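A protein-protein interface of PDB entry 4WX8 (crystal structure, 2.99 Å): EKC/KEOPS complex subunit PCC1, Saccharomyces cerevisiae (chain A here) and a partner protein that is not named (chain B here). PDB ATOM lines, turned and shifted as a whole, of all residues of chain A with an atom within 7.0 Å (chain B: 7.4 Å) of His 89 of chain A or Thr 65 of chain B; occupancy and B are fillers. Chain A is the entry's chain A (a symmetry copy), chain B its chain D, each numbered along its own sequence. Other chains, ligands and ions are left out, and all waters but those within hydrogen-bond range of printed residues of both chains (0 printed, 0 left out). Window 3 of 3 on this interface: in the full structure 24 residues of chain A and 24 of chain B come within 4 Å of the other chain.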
ATOM      1  N   GLU A  20     -22.473  18.147   6.673  1.00  0.00           N
ATOM      2  CA  GLU A  20     -22.038  16.916   6.063  1.00  0.00           C
ATOM      3  C   GLU A  20     -23.205  15.947   5.907  1.00  0.00           C
ATOM      4  O   GLU A  20     -23.275  15.177   4.931  1.00  0.00           O
ATOM      5  CB  GLU A  20     -20.904  16.314   6.893  1.00  0.00           C
ATOM      6  CG  GLU A  20     -19.671  17.217   6.995  1.00  0.00           C
ATOM      7  CD  GLU A  20     -18.456  16.457   7.490  1.00  0.00           C
ATOM      8  OE1 GLU A  20     -17.826  15.756   6.669  1.00  0.00           O
ATOM      9  OE2 GLU A  20     -18.138  16.528   8.704  1.00  0.00           O
ATOM     10  N   MET A  84     -19.549  21.408  16.550  1.00  0.00           N
ATOM     11  CA  MET A  84     -19.628  20.146  15.818  1.00  0.00           C
ATOM     12  C   MET A  84     -18.316  19.822  15.193  1.00  0.00           C
ATOM     13  O   MET A  84     -18.077  18.682  14.842  1.00  0.00           O
ATOM     14  CB  MET A  84     -20.641  20.192  14.695  1.00  0.00           C
ATOM     15  CG  MET A  84     -21.986  20.518  15.302  1.00  0.00           C
ATOM     16  SD  MET A  84     -23.433  20.036  14.069  1.00  0.00           S
ATOM     17  CE  MET A  84     -23.326  18.098  14.406  1.00  0.00           C
ATOM     18  N   ASP A  85     -17.452  20.824  15.016  1.00  0.00           N
ATOM     19  CA  ASP A  85     -16.147  20.566  14.427  1.00  0.00           C
ATOM     20  C   ASP A  85     -15.332  19.825  15.476  1.00  0.00           C
ATOM     21  O   ASP A  85     -14.929  18.679  15.253  1.00  0.00           O
ATOM     22  CB  ASP A  85     -15.472  21.858  13.948  1.00  0.00           C
ATOM     23  CG  ASP A  85     -14.207  21.608  13.090  1.00  0.00           C
ATOM     24  OD1 ASP A  85     -13.980  20.478  12.619  1.00  0.00           O
ATOM     25  OD2 ASP A  85     -13.419  22.563  12.889  1.00  0.00           O
ATOM     26  N   VAL A  86     -15.147  20.428  16.645  1.00  0.00           N
ATOM     27  CA  VAL A  86     -14.309  19.758  17.640  1.00  0.00           C
ATOM     28  C   VAL A  86     -14.800  18.344  18.026  1.00  0.00           C
ATOM     29  O   VAL A  86     -13.980  17.455  18.206  1.00  0.00           O
ATOM     30  CB  VAL A  86     -14.032  20.613  18.898  1.00  0.00           C
ATOM     31  CG1 VAL A  86     -13.726  22.033  18.495  1.00  0.00           C
ATOM     32  CG2 VAL A  86     -15.188  20.573  19.869  1.00  0.00           C
ATOM     33  N   LEU A  87     -16.121  18.168  18.149  1.00  0.00           N
ATOM     34  CA  LEU A  87     -16.734  16.880  18.531  1.00  0.00           C
ATOM     35  C   LEU A  87     -16.547  15.825  17.429  1.00  0.00           C
ATOM     36  O   LEU A  87     -16.053  14.727  17.687  1.00  0.00           O
ATOM     37  CB  LEU A  87     -18.226  17.042  18.887  1.00  0.00           C
ATOM     38  CG  LEU A  87     -18.587  17.479  20.317  1.00  0.00           C
ATOM     39  N   SER A  88     -16.901  16.195  16.204  1.00  0.00           N
ATOM     40  CA  SER A  88     -16.743  15.360  15.015  1.00  0.00           C
ATOM     41  C   SER A  88     -15.346  14.736  14.834  1.00  0.00           C
ATOM     42  O   SER A  88     -15.192  13.746  14.109  1.00  0.00           O
ATOM     43  CB  SER A  88     -17.063  16.241  13.807  1.00  0.00           C
ATOM     44  OG  SER A  88     -16.836  15.597  12.574  1.00  0.00           O
ATOM     45  N   HIS A  89     -14.337  15.309  15.485  1.00  0.00           N
ATOM     46  CA  HIS A  89     -12.939  14.904  15.259  1.00  0.00           C
ATOM     47  C   HIS A  89     -12.356  14.363  16.533  1.00  0.00           C
ATOM     48  O   HIS A  89     -11.386  13.625  16.519  1.00  0.00           O
ATOM     49  CB  HIS A  89     -12.104  16.099  14.720  1.00  0.00           C
ATOM     50  CG  HIS A  89     -12.483  16.490  13.324  1.00  0.00           C
ATOM     51  ND1 HIS A  89     -13.394  17.482  13.050  1.00  0.00           N
ATOM     52  CD2 HIS A  89     -12.156  15.942  12.130  1.00  0.00           C
ATOM     53  CE1 HIS A  89     -13.583  17.555  11.746  1.00  0.00           C
ATOM     54  NE2 HIS A  89     -12.844  16.629  11.164  1.00  0.00           N
ATOM     55  N   HIS A  90     -12.972  14.757  17.639  1.00  0.00           N
ATOM     56  CA  HIS A  90     -12.654  14.218  18.954  1.00  0.00           C
ATOM     57  C   HIS A  90     -11.542  15.030  19.679  1.00  0.00           C
ATOM     58  O   HIS A  90     -10.347  14.738  19.585  1.00  0.00           O
ATOM     59  CB  HIS A  90     -12.373  12.695  18.850  1.00  0.00           C
ATOM     60  CG  HIS A  90     -13.466  11.937  18.147  1.00  0.00           C
ATOM     61  ND1 HIS A  90     -14.718  11.761  18.699  1.00  0.00           N
ATOM     62  CD2 HIS A  90     -13.512  11.354  16.924  1.00  0.00           C
ATOM     63  CE1 HIS A  90     -15.487  11.097  17.854  1.00  0.00           C
ATOM     64  NE2 HIS A  90     -14.781  10.839  16.768  1.00  0.00           N
ATOM     65  N   GLN B  63      -5.152  19.202   6.949  1.00  0.00           N
ATOM     66  CA  GLN B  63      -5.226  20.666   7.076  1.00  0.00           C
ATOM     67  C   GLN B  63      -6.602  21.043   7.641  1.00  0.00           C
ATOM     68  O   GLN B  63      -7.151  20.319   8.485  1.00  0.00           O
ATOM     69  CB  GLN B  63      -4.966  21.352   5.717  1.00  0.00           C
ATOM     70  N   LEU B  64      -7.169  22.153   7.169  1.00  0.00           N
ATOM     71  CA  LEU B  64      -8.487  22.602   7.643  1.00  0.00           C
ATOM     72  C   LEU B  64      -9.606  21.582   7.343  1.00  0.00           C
ATOM     73  O   LEU B  64      -9.587  20.890   6.322  1.00  0.00           O
ATOM     74  CB  LEU B  64      -8.827  23.977   7.042  1.00  0.00           C
ATOM     75  CG  LEU B  64      -9.792  24.862   7.841  1.00  0.00           C
ATOM     76  CD1 LEU B  64      -9.417  24.962   9.312  1.00  0.00           C
ATOM     77  CD2 LEU B  64      -9.841  26.253   7.236  1.00  0.00           C
ATOM     78  N   THR B  65     -10.582  21.488   8.239  1.00  0.00           N
ATOM     79  CA  THR B  65     -11.630  20.481   8.121  1.00  0.00           C
ATOM     80  C   THR B  65     -12.805  21.028   7.324  1.00  0.00           C
ATOM     81  O   THR B  65     -13.011  22.236   7.258  1.00  0.00           O
ATOM     82  CB  THR B  65     -12.135  20.050   9.509  1.00  0.00           C
ATOM     83  OG1 THR B  65     -12.768  21.152  10.157  1.00  0.00           O
ATOM     84  CG2 THR B  65     -11.014  19.632  10.379  1.00  0.00           C
ATOM     85  N   TYR B  66     -13.587  20.131   6.731  1.00  0.00           N
ATOM     86  CA  TYR B  66     -14.862  20.508   6.127  1.00  0.00           C
ATOM     87  C   TYR B  66     -15.549  21.631   6.919  1.00  0.00           C
ATOM     88  O   TYR B  66     -15.562  22.781   6.485  1.00  0.00           O
ATOM     89  CB  TYR B  66     -15.805  19.305   6.028  1.00  0.00           C
ATOM     90  CG  TYR B  66     -17.109  19.683   5.375  1.00  0.00           C
ATOM     91  CD1 TYR B  66     -17.243  19.662   3.993  1.00  0.00           C
ATOM     92  CD2 TYR B  66     -18.189  20.110   6.128  1.00  0.00           C
ATOM     93  CE1 TYR B  66     -18.424  20.032   3.381  1.00  0.00           C
ATOM     94  CE2 TYR B  66     -19.375  20.492   5.524  1.00  0.00           C
ATOM     95  CZ  TYR B  66     -19.491  20.446   4.154  1.00  0.00           C
ATOM     96  OH  TYR B  66     -20.676  20.824   3.554  1.00  0.00           O
ATOM     97  N   LEU B  67     -16.102  21.292   8.084  1.00  0.00           N
ATOM     98  CA  LEU B  67     -16.808  22.272   8.927  1.00  0.00           C
ATOM     99  C   LEU B  67     -15.951  23.477   9.313  1.00  0.00           C
ATOM    100  O   LEU B  67     -16.464  24.577   9.553  1.00  0.00           O
ATOM    101  CB  LEU B  67     -17.268  21.610  10.229  1.00  0.00           C
ATOM    102  CG  LEU B  67     -18.228  20.456  10.105  1.00  0.00           C
ATOM    103  CD1 LEU B  67     -18.335  19.833  11.477  1.00  0.00           C
ATOM    104  CD2 LEU B  67     -19.567  20.926   9.612  1.00  0.00           C
ATOM    105  N   GLY B  68     -14.655  23.227   9.444  1.00  0.00           N
ATOM    106  CA  GLY B  68     -13.706  24.287   9.661  1.00  0.00           C
ATOM    107  C   GLY B  68     -13.837  25.258   8.522  1.00  0.00           C
ATOM    108  O   GLY B  68     -14.002  26.443   8.754  1.00  0.00           O
ATOM    109  N   GLN B  69     -13.799  24.752   7.292  1.00  0.00           N
ATOM    110  CA  GLN B  69     -13.914  25.610   6.131  1.00  0.00           C
ATOM    111  C   GLN B  69     -15.280  26.288   6.161  1.00  0.00           C
ATOM    112  O   GLN B  69     -15.397  27.493   5.997  1.00  0.00           O
ATOM    113  CB  GLN B  69     -13.721  24.812   4.836  1.00  0.00           C
ATOM    114  CG  GLN B  69     -12.299  24.327   4.582  1.00  0.00           C
ATOM    115  N   LEU B  70     -16.317  25.507   6.410  1.00  0.00           N
ATOM    116  CA  LEU B  70     -17.667  26.033   6.473  1.00  0.00           C
ATOM    117  C   LEU B  70     -17.714  27.252   7.389  1.00  0.00           C
ATOM    118  O   LEU B  70     -18.350  28.252   7.073  1.00  0.00           O
ATOM    119  CB  LEU B  70     -18.606  24.939   6.994  1.00  0.00           C
ATOM    120  CG  LEU B  70     -20.098  25.252   7.149  1.00  0.00           C
ATOM    121  CD1 LEU B  70     -20.678  25.912   5.904  1.00  0.00           C
ATOM    122  CD2 LEU B  70     -20.870  23.987   7.474  1.00  0.00           C
ATOM    123  N   ARG B  71     -17.031  27.176   8.525  1.00  0.00           N
ATOM    124  CA  ARG B  71     -17.111  28.248   9.498  1.00  0.00           C
ATOM    125  C   ARG B  71     -16.579  29.510   8.877  1.00  0.00           C
ATOM    126  O   ARG B  71     -17.121  30.586   9.127  1.00  0.00           O
ATOM    127  CB  ARG B  71     -16.352  27.927  10.795  1.00  0.00           C
ATOM    128  CG  ARG B  71     -16.832  28.749  11.983  1.00  0.00           C
ATOM    129  CD  ARG B  71     -16.181  28.370  13.305  1.00  0.00           C
ATOM    130  NE  ARG B  71     -14.884  29.021  13.520  1.00  0.00           N
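A ring nitrogen (ND1) of His 89 of chain A lies within hydrogen-bond range of the backbone carbonyl oxygen (O) of Asp 85 of chain A (2.9 Å). The side-chain hydroxyl (OG1) of Thr 65 of chain B is in hydrogen-bond range of the backbone NH (N) of Gly 68 of chain B.
His 89 of chain A touches just one residue of chain B: Thr 65 (3.6 Å). Of chain A, only Asp 85 (2.8 Å) and His 89 (3.6 Å) come within 4 Å of Thr 65 of chain B. Printed residues of chain A within 4 Å of Gly 68 of chain B: Asp 85 (3.7 Å). Of the printed residues of chain B, Glu 20 of chain A touches Tyr 66. His 90 of chain A touches none of the printed residues of chain B. Leu 87 of chain A touches none of the printed residues of chain B. The nearest residue of chain B that does not touch His 89 of chain A is Leu 67 of chain B (5.3 Å). The nearest residue of chain A that does not touch Thr 65 of chain B is Val 86 of chain A (6.9 Å).
Hydrophobic or aromatic side chains of chain B within 4 Å of the printed part of chain A: Tyr 66 and Leu 67. Of the 8 printed residues of chain A, 4 touch a printed residue of chain B.
Among the printed residues, merely in contact across the chains: Glu 20 of chain A with Tyr 66 of chain B, Met 84 of chain A with Leu 67 of chain B, Asp 85 of chain A with Leu 67 of chain B, Asp 85 of chain A with Gly 68 of chain B and His 89 of chain A with Thr 65 of chain B.
The side-chain hydroxyl (OG1) of Thr 65 of chain B sits at hydrogen-bond distance from the side-chain carboxylate (OD1) of Asp 85 of chain A (2.8 Å).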
